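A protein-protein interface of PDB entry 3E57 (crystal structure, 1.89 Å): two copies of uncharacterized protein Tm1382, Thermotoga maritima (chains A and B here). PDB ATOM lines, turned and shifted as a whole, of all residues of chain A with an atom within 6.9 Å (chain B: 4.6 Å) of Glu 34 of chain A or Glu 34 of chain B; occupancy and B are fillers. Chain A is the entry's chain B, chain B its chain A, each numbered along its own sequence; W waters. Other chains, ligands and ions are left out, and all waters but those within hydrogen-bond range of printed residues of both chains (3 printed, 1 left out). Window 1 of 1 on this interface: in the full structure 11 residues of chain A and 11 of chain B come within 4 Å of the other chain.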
ATOM      1  N   GLU A  32      16.454 -11.893 -25.400  1.00  0.00           N
ATOM      2  CA  GLU A  32      17.639 -12.525 -25.936  1.00  0.00           C
ATOM      3  C   GLU A  32      17.941 -13.792 -25.152  1.00  0.00           C
ATOM      4  O   GLU A  32      18.277 -13.728 -23.972  1.00  0.00           O
ATOM      5  CB  GLU A  32      18.813 -11.557 -25.827  1.00  0.00           C
ATOM      6  CG  GLU A  32      18.634 -10.330 -26.722  1.00  0.00           C
ATOM      7  CD  GLU A  32      19.628  -9.222 -26.419  1.00  0.00           C
ATOM      8  OE1 GLU A  32      20.856  -9.475 -26.470  1.00  0.00           O
ATOM      9  OE2 GLU A  32      19.173  -8.086 -26.148  1.00  0.00           O
ATOM     10  N   PHE A  33      17.820 -14.938 -25.807  1.00  0.00           N
ATOM     11  CA  PHE A  33      18.216 -16.194 -25.182  1.00  0.00           C
ATOM     12  C   PHE A  33      18.830 -17.125 -26.203  1.00  0.00           C
ATOM     13  O   PHE A  33      18.611 -16.961 -27.393  1.00  0.00           O
ATOM     14  CB  PHE A  33      17.026 -16.859 -24.486  1.00  0.00           C
ATOM     15  CG  PHE A  33      15.925 -17.282 -25.409  1.00  0.00           C
ATOM     16  CD1 PHE A  33      15.760 -18.616 -25.753  1.00  0.00           C
ATOM     17  CD2 PHE A  33      15.028 -16.350 -25.914  1.00  0.00           C
ATOM     18  CE1 PHE A  33      14.730 -19.004 -26.581  1.00  0.00           C
ATOM     19  CE2 PHE A  33      14.003 -16.730 -26.738  1.00  0.00           C
ATOM     20  CZ  PHE A  33      13.844 -18.063 -27.077  1.00  0.00           C
ATOM     21  N   GLU A  34      19.600 -18.085 -25.711  1.00  0.00           N
ATOM     22  CA  GLU A  34      20.278 -19.079 -26.540  1.00  0.00           C
ATOM     23  C   GLU A  34      19.937 -20.431 -25.958  1.00  0.00           C
ATOM     24  O   GLU A  34      20.375 -20.751 -24.871  1.00  0.00           O
ATOM     25  CB  GLU A  34      21.795 -18.850 -26.486  1.00  0.00           C
ATOM     26  CG  GLU A  34      22.647 -19.893 -27.219  1.00  0.00           C
ATOM     27  CD  GLU A  34      22.574 -19.773 -28.742  1.00  0.00           C
ATOM     28  OE1 GLU A  34      22.480 -18.631 -29.253  1.00  0.00           O
ATOM     29  OE2 GLU A  34      22.628 -20.832 -29.420  1.00  0.00           O
ATOM     30  N   GLY A  35      19.140 -21.209 -26.674  1.00  0.00           N
ATOM     31  CA  GLY A  35      18.716 -22.514 -26.182  1.00  0.00           C
ATOM     32  C   GLY A  35      17.211 -22.595 -26.174  1.00  0.00           C
ATOM     33  O   GLY A  35      16.583 -22.360 -27.193  1.00  0.00           O
ATOM     34  N   PHE A  36      16.635 -22.916 -25.018  1.00  0.00           N
ATOM     35  CA  PHE A  36      15.192 -23.045 -24.879  1.00  0.00           C
ATOM     36  C   PHE A  36      14.708 -22.125 -23.776  1.00  0.00           C
ATOM     37  O   PHE A  36      15.399 -21.941 -22.779  1.00  0.00           O
ATOM     38  CB  PHE A  36      14.826 -24.482 -24.525  1.00  0.00           C
ATOM     39  CG  PHE A  36      13.439 -24.653 -23.973  1.00  0.00           C
ATOM     40  CD1 PHE A  36      12.366 -24.872 -24.818  1.00  0.00           C
ATOM     41  CD2 PHE A  36      13.210 -24.602 -22.600  1.00  0.00           C
ATOM     42  CE1 PHE A  36      11.071 -25.044 -24.304  1.00  0.00           C
ATOM     43  CE2 PHE A  36      11.934 -24.773 -22.079  1.00  0.00           C
ATOM     44  CZ  PHE A  36      10.860 -24.993 -22.936  1.00  0.00           C
ATOM     45  N   MET A  37      13.515 -21.573 -23.963  1.00  0.00           N
ATOM     46  CA  MET A  37      12.821 -20.792 -22.921  1.00  0.00           C
ATOM     47  C   MET A  37      11.330 -21.117 -22.900  1.00  0.00           C
ATOM     48  O   MET A  37      10.683 -21.112 -23.947  1.00  0.00           O
ATOM     49  CB  MET A  37      12.987 -19.298 -23.182  1.00  0.00           C
ATOM     50  CG  MET A  37      12.390 -18.448 -22.064  1.00  0.00           C
ATOM     51  SD  MET A  37      12.719 -16.706 -22.262  1.00  0.00           S
ATOM     52  CE  MET A  37      11.867 -16.391 -23.783  1.00  0.00           C
ATOM     53  N   ARG A  38      10.798 -21.406 -21.709  1.00  0.00           N
ATOM     54  CA  ARG A  38       9.375 -21.653 -21.521  1.00  0.00           C
ATOM     55  C   ARG A  38       8.629 -20.364 -21.774  1.00  0.00           C
ATOM     56  O   ARG A  38       9.059 -19.315 -21.307  1.00  0.00           O
ATOM     57  CB  ARG A  38       9.080 -22.121 -20.100  1.00  0.00           C
ATOM     58  CG  ARG A  38       7.586 -22.218 -19.758  1.00  0.00           C
ATOM     59  CD  ARG A  38       7.266 -23.481 -19.001  1.00  0.00           C
ATOM     60  NE  ARG A  38       7.722 -24.581 -19.850  1.00  0.00           N
ATOM     61  CZ  ARG A  38       7.202 -25.798 -19.936  1.00  0.00           C
ATOM     62  NH1 ARG A  38       6.145 -26.179 -19.214  1.00  0.00           N
ATOM     63  NH2 ARG A  38       7.777 -26.641 -20.773  1.00  0.00           N
ATOM     64  N   ASN A 145      15.633 -21.173 -29.666  1.00  0.00           N
ATOM     65  CA  ASN A 145      16.334 -20.166 -30.435  1.00  0.00           C
ATOM     66  C   ASN A 145      17.808 -20.400 -30.244  1.00  0.00           C
ATOM     67  O   ASN A 145      18.350 -20.132 -29.174  1.00  0.00           O
ATOM     68  CB  ASN A 145      15.947 -18.759 -29.957  1.00  0.00           C
ATOM     69  CG  ASN A 145      16.562 -17.658 -30.798  1.00  0.00           C
ATOM     70  OD1 ASN A 145      16.521 -17.708 -32.024  1.00  0.00           O
ATOM     71  ND2 ASN A 145      17.126 -16.650 -30.144  1.00  0.00           N
ATOM     72  N   SER A 146      18.457 -20.964 -31.254  1.00  0.00           N
ATOM     73  CA  SER A 146      19.887 -21.241 -31.162  1.00  0.00           C
ATOM     74  C   SER A 146      20.580 -20.673 -32.372  1.00  0.00           C
ATOM     75  O   SER A 146      19.996 -20.599 -33.450  1.00  0.00           O
ATOM     76  CB  SER A 146      20.153 -22.734 -31.093  1.00  0.00           C
ATOM     77  OG  SER A 146      19.622 -23.352 -32.235  1.00  0.00           O
ATOM     78  N   SER A 147      21.831 -20.278 -32.188  1.00  0.00           N
ATOM     79  CA  SER A 147      22.533 -19.531 -33.200  1.00  0.00           C
ATOM     80  C   SER A 147      23.769 -20.276 -33.684  1.00  0.00           C
ATOM     81  O   SER A 147      24.627 -19.674 -34.323  1.00  0.00           O
ATOM     82  CB  SER A 147      22.938 -18.167 -32.643  1.00  0.00           C
ATOM     83  OG  SER A 147      23.855 -18.317 -31.575  1.00  0.00           O
ATOM     84  N   THR A 148      23.855 -21.576 -33.413  1.00  0.00           N
ATOM     85  CA  THR A 148      25.091 -22.320 -33.691  1.00  0.00           C
ATOM     86  C   THR A 148      25.277 -22.765 -35.158  1.00  0.00           C
ATOM     87  O   THR A 148      26.352 -23.248 -35.521  1.00  0.00           O
ATOM     88  CB  THR A 148      25.251 -23.532 -32.751  1.00  0.00           C
ATOM     89  OG1 THR A 148      24.070 -24.336 -32.779  1.00  0.00           O
ATOM     90  CG2 THR A 148      25.495 -23.059 -31.324  1.00  0.00           C
ATOM     91  N   SER A 152      19.986 -22.750 -38.019  1.00  0.00           N
ATOM     92  CA  SER A 152      19.508 -22.382 -36.684  1.00  0.00           C
ATOM     93  C   SER A 152      19.195 -20.905 -36.553  1.00  0.00           C
ATOM     94  O   SER A 152      18.152 -20.541 -36.007  1.00  0.00           O
ATOM     95  CB  SER A 152      20.542 -22.766 -35.624  1.00  0.00           C
ATOM     96  OG  SER A 152      20.605 -24.166 -35.535  1.00  0.00           O
ATOM     97  N   LYS A 197      19.318 -32.108 -29.404  1.00  0.00           N
ATOM     98  CA  LYS A 197      20.037 -32.107 -28.146  1.00  0.00           C
ATOM     99  C   LYS A 197      19.344 -31.189 -27.124  1.00  0.00           C
ATOM    100  O   LYS A 197      19.216 -31.522 -25.932  1.00  0.00           O
ATOM    101  CB  LYS A 197      21.467 -31.633 -28.380  1.00  0.00           C
ATOM    102  CG  LYS A 197      22.420 -31.932 -27.267  1.00  0.00           C
ATOM    103  CD  LYS A 197      23.821 -31.514 -27.666  1.00  0.00           C
ATOM    104  CE  LYS A 197      24.817 -32.000 -26.631  1.00  0.00           C
ATOM    105  NZ  LYS A 197      25.103 -33.479 -26.760  1.00  0.00           N
ATOM    106  N   ILE A 198      18.906 -30.032 -27.589  1.00  0.00           N
ATOM    107  CA  ILE A 198      18.273 -29.063 -26.689  1.00  0.00           C
ATOM    108  C   ILE A 198      16.976 -29.644 -26.169  1.00  0.00           C
ATOM    109  O   ILE A 198      16.698 -29.584 -24.970  1.00  0.00           O
ATOM    110  CB  ILE A 198      17.985 -27.731 -27.398  1.00  0.00           C
ATOM    111  CG1 ILE A 198      19.294 -26.993 -27.733  1.00  0.00           C
ATOM    112  CG2 ILE A 198      17.114 -26.839 -26.499  1.00  0.00           C
ATOM    113  CD1 ILE A 198      19.131 -25.890 -28.758  1.00  0.00           C
ATOM    114  N   ALA A 201      17.337 -32.290 -23.488  1.00  0.00           N
ATOM    115  CA  ALA A 201      17.598 -31.689 -22.199  1.00  0.00           C
ATOM    116  C   ALA A 201      16.301 -31.164 -21.558  1.00  0.00           C
ATOM    117  O   ALA A 201      16.067 -31.372 -20.367  1.00  0.00           O
ATOM    118  CB  ALA A 201      18.663 -30.578 -22.326  1.00  0.00           C
ATOM    119  N   VAL A 202      15.441 -30.533 -22.359  1.00  0.00           N
ATOM    120  CA  VAL A 202      14.173 -29.971 -21.867  1.00  0.00           C
ATOM    121  C   VAL A 202      13.268 -31.083 -21.364  1.00  0.00           C
ATOM    122  O   VAL A 202      12.726 -31.015 -20.251  1.00  0.00           O
ATOM    123  CB  VAL A 202      13.459 -29.142 -22.973  1.00  0.00           C
ATOM    124  CG1 VAL A 202      12.028 -28.761 -22.548  1.00  0.00           C
ATOM    125  CG2 VAL A 202      14.287 -27.894 -23.310  1.00  0.00           C
ATOM    126  N   ASN A 205      14.504 -32.738 -18.124  1.00  0.00           N
ATOM    127  CA  ASN A 205      14.260 -31.864 -16.969  1.00  0.00           C
ATOM    128  C   ASN A 205      12.776 -31.749 -16.609  1.00  0.00           C
ATOM    129  O   ASN A 205      12.435 -31.599 -15.432  1.00  0.00           O
ATOM    130  CB  ASN A 205      14.871 -30.473 -17.171  1.00  0.00           C
ATOM    131  CG  ASN A 205      15.322 -29.841 -15.858  1.00  0.00           C
ATOM    132  OD1 ASN A 205      16.031 -30.464 -15.058  1.00  0.00           O
ATOM    133  ND2 ASN A 205      14.932 -28.602 -15.641  1.00  0.00           N
ATOM    134  N   PHE B  33      14.344 -22.012 -18.304  1.00  0.00           N
ATOM    135  CA  PHE B  33      15.122 -21.968 -19.534  1.00  0.00           C
ATOM    136  C   PHE B  33      16.310 -22.888 -19.443  1.00  0.00           C
ATOM    137  O   PHE B  33      16.762 -23.248 -18.345  1.00  0.00           O
ATOM    138  CB  PHE B  33      15.570 -20.543 -19.876  1.00  0.00           C
ATOM    139  CG  PHE B  33      16.557 -19.954 -18.904  1.00  0.00           C
ATOM    140  CD1 PHE B  33      17.899 -19.840 -19.230  1.00  0.00           C
ATOM    141  CD2 PHE B  33      16.131 -19.467 -17.677  1.00  0.00           C
ATOM    142  CE1 PHE B  33      18.791 -19.267 -18.354  1.00  0.00           C
ATOM    143  CE2 PHE B  33      17.017 -18.904 -16.802  1.00  0.00           C
ATOM    144  CZ  PHE B  33      18.376 -18.810 -17.145  1.00  0.00           C
ATOM    145  N   GLU B  34      16.809 -23.244 -20.614  1.00  0.00           N
ATOM    146  CA  GLU B  34      17.897 -24.197 -20.756  1.00  0.00           C
ATOM    147  C   GLU B  34      18.892 -23.566 -21.716  1.00  0.00           C
ATOM    148  O   GLU B  34      18.608 -23.432 -22.899  1.00  0.00           O
ATOM    149  CB  GLU B  34      17.321 -25.526 -21.263  1.00  0.00           C
ATOM    150  CG  GLU B  34      18.327 -26.663 -21.513  1.00  0.00           C
ATOM    151  CD  GLU B  34      18.909 -27.267 -20.241  1.00  0.00           C
ATOM    152  OE1 GLU B  34      18.171 -27.440 -19.245  1.00  0.00           O
ATOM    153  OE2 GLU B  34      20.117 -27.594 -20.255  1.00  0.00           O
ATOM    154  N   GLY B  35      20.033 -23.135 -21.192  1.00  0.00           N
ATOM    155  CA  GLY B  35      21.045 -22.444 -21.976  1.00  0.00           C
ATOM    156  C   GLY B  35      21.350 -21.081 -21.368  1.00  0.00           C
ATOM    157  O   GLY B  35      21.666 -21.000 -20.179  1.00  0.00           O
ATOM    158  N   PHE B  36      21.237 -20.013 -22.168  1.00  0.00           N
ATOM    159  CA  PHE B  36      21.556 -18.662 -21.708  1.00  0.00           C
ATOM    160  C   PHE B  36      20.359 -17.734 -21.890  1.00  0.00           C
ATOM    161  O   PHE B  36      19.621 -17.847 -22.851  1.00  0.00           O
ATOM    162  CB  PHE B  36      22.762 -18.120 -22.485  1.00  0.00           C
ATOM    163  CG  PHE B  36      22.928 -16.613 -22.410  1.00  0.00           C
ATOM    164  CD1 PHE B  36      23.695 -16.029 -21.410  1.00  0.00           C
ATOM    165  CD2 PHE B  36      22.340 -15.784 -23.359  1.00  0.00           C
ATOM    166  CE1 PHE B  36      23.857 -14.655 -21.354  1.00  0.00           C
ATOM    167  CE2 PHE B  36      22.506 -14.403 -23.295  1.00  0.00           C
ATOM    168  CZ  PHE B  36      23.263 -13.852 -22.294  1.00  0.00           C
ATOM    169  N   ASN B 145      21.852 -21.393 -17.341  1.00  0.00           N
ATOM    170  CA  ASN B 145      21.153 -22.442 -16.592  1.00  0.00           C
ATOM    171  C   ASN B 145      21.023 -23.665 -17.487  1.00  0.00           C
ATOM    172  O   ASN B 145      20.309 -23.641 -18.497  1.00  0.00           O
ATOM    173  CB  ASN B 145      19.754 -22.006 -16.144  1.00  0.00           C
ATOM    174  CG  ASN B 145      19.088 -23.030 -15.235  1.00  0.00           C
ATOM    175  OD1 ASN B 145      19.720 -23.550 -14.319  1.00  0.00           O
ATOM    176  ND2 ASN B 145      17.805 -23.302 -15.465  1.00  0.00           N
ATOM    177  N   SER B 146      21.707 -24.746 -17.120  1.00  0.00           N
ATOM    178  CA  SER B 146      21.646 -25.954 -17.910  1.00  0.00           C
ATOM    179  C   SER B 146      21.475 -27.146 -16.992  1.00  0.00           C
ATOM    180  O   SER B 146      21.800 -27.095 -15.824  1.00  0.00           O
ATOM    181  CB  SER B 146      22.887 -26.105 -18.768  1.00  0.00           C
ATOM    182  OG  SER B 146      24.040 -26.133 -17.945  1.00  0.00           O
ATOM    183  N   SER B 147      20.887 -28.199 -17.519  1.00  0.00           N
ATOM    184  CA  SER B 147      20.478 -29.304 -16.672  1.00  0.00           C
ATOM    185  C   SER B 147      21.079 -30.618 -17.126  1.00  0.00           C
ATOM    186  O   SER B 147      20.614 -31.682 -16.713  1.00  0.00           O
ATOM    187  CB  SER B 147      18.960 -29.406 -16.723  1.00  0.00           C
ATOM    188  OG  SER B 147      18.559 -29.745 -18.028  1.00  0.00           O
ATOM    189  N   THR B 148      22.106 -30.562 -17.960  1.00  0.00           N
ATOM    190  CA  THR B 148      22.567 -31.764 -18.634  1.00  0.00           C
ATOM    191  C   THR B 148      23.574 -32.582 -17.822  1.00  0.00           C
ATOM    192  O   THR B 148      23.873 -33.708 -18.197  1.00  0.00           O
ATOM    193  CB  THR B 148      23.147 -31.436 -20.000  1.00  0.00           C
ATOM    194  OG1 THR B 148      24.158 -30.449 -19.856  1.00  0.00           O
ATOM    195  CG2 THR B 148      22.041 -30.890 -20.933  1.00  0.00           C
ATOM    196  N   ALA B 201      28.724 -19.747 -27.978  1.00  0.00           N
ATOM    197  CA  ALA B 201      27.590 -19.394 -28.838  1.00  0.00           C
ATOM    198  C   ALA B 201      27.138 -17.970 -28.603  1.00  0.00           C
ATOM    199  O   ALA B 201      26.925 -17.214 -29.559  1.00  0.00           O
ATOM    200  CB  ALA B 201      26.423 -20.372 -28.639  1.00  0.00           C
ATOM    201  N   VAL B 202      27.021 -17.596 -27.331  1.00  0.00           N
ATOM    202  CA  VAL B 202      26.587 -16.254 -26.938  1.00  0.00           C
ATOM    203  C   VAL B 202      27.560 -15.173 -27.391  1.00  0.00           C
ATOM    204  O   VAL B 202      27.143 -14.164 -27.975  1.00  0.00           O
ATOM    205  CB  VAL B 202      26.393 -16.140 -25.398  1.00  0.00           C
ATOM    206  CG1 VAL B 202      26.128 -14.670 -24.977  1.00  0.00           C
ATOM    207  CG2 VAL B 202      25.270 -17.059 -24.935  1.00  0.00           C
HETATM  208  O   HOH W   1      18.122 -32.118 -18.611  1.00  0.00           O
HETATM  209  O   HOH W   2      17.503 -33.004 -16.000  1.00  0.00           O
HETATM  210  O   HOH W   3      26.479 -18.229 -32.063  1.00  0.00           O
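O of Phe 36 of chain A is in hydrogen-bond range of N of Glu 34 of chain B (2.9 Å).
O of Phe 36 of chain B sits at hydrogen-bond distance from N of Glu 34 of chain A (2.9 Å).
O of Asn 145 of chain A sits at hydrogen-bond distance from N of Gly 35 of chain A, 2.8 Å away.
N of Gly 35 of chain B is in hydrogen-bond range of O of Asn 145 of chain B (2.8 Å).
O of Phe 33 of chain B is in hydrogen-bond range of ND2 of Asn 145 of chain B, at 3.1 Å.
The side-chain carboxylate (OE1) of Glu 34 of chain B lies within hydrogen-bond range of the side-chain hydroxyl (OG) of Ser 147 of chain B (2.6 Å).
The side-chain carboxylate (OE1) of Glu 34 of chain A sits at hydrogen-bond distance from the side-chain hydroxyl (OG) of Ser 147 of chain A.
The backbone carbonyl oxygen (O) of Phe 33 of chain A is in hydrogen-bond range of the side-chain amide nitrogen (ND2) of Asn 145 of chain A (3.1 Å).
Among the printed residues, merely in contact across the chains: Phe 33 of chain A with Phe 36 of chain B (3.2 Å), Glu 34 of chain A with Glu 34 of chain B (3.8 Å), Glu 34 of chain A with Gly 35 of chain B (3.4 Å), Glu 34 of chain A with Ala 201 of chain B (3.9 Å), Gly 35 of chain A with Glu 34 of chain B (3.4 Å), Phe 36 of chain A with Phe 33 of chain B (3.2 Å), Ser 147 of chain A with Ala 201 of chain B (3.8 Å), Thr 148 of chain A with Ala 201 of chain B (3.9 Å), Ala 201 of chain A with Glu 34 of chain B (3.9 Å), Ala 201 of chain A with Ser 147 of chain B (3.8 Å), Ala 201 of chain A with Thr 148 of chain B (3.7 Å) and Asn 205 of chain A with Ser 147 of chain B (3.5 Å).
Glu 34 of chain B touches four residues of chain A.
Of the printed residues of chain A, Ser 147 of chain B touches Ala 201 and Asn 205.
Of the printed residues of chain B, Phe 36 of chain A touches Phe 33 (3.2 Å) and Glu 34 (2.9 Å).
Printed residues of chain B within 4 Å of Gly 35 of chain A: Glu 34.
Of the printed residues of chain A, Ala 201 of chain B touches Glu 34, Ser 147 and Thr 148.
Lys 197 of chain A touches none of the printed residues of chain B.
Ser 146 of chain B touches none of the printed residues of chain A.
Printed residues of chain B that touch a printed residue of chain A: Phe 33, Glu 34, Gly 35, Phe 36, Ser 147, Thr 148 and Ala 201.
Hydrophobic or aromatic side chains of chain B that line the printed part of chain A: Phe 33 and Ala 201.
Hydrophobic or aromatic side chains of chain A that line the printed part of chain B: Phe 33 and Ala 201.
Among the printed residues, 14 pairs touch across the chains.
Phe 33 of chain A touches Phe 36 of chain B, and with the chains exchanged Phe 36 of chain A touches Phe 33 of chain B.
Glu 34 of chain A touches Gly 35 of chain B, and with the chains exchanged Gly 35 of chain A touches Glu 34 of chain B.
Glu 34 of chain A touches Ala 201 of chain B, and with the chains exchanged Ala 201 of chain A touches Glu 34 of chain B.
Ser 147 of chain A touches Ala 201 of chain B, and with the chains exchanged Ala 201 of chain A touches Ser 147 of chain B.
10 positions are printed for both chains.
Water W1 bridges the side-chain hydroxyl (OG) of Ser 147 of chain B (2.5 Å) and the backbone carbonyl oxygen (O) of Ala 201 of chain A (2.8 Å).
Water W3 lies within hydrogen-bond range of OG of Ser 147 of chain A (2.7 Å) and O of Ala 201 of chain B (2.7 Å).
Water W2 lies within hydrogen-bond range of OD1 of Asn 205 of chain A and O of Ser 147 of chain B.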
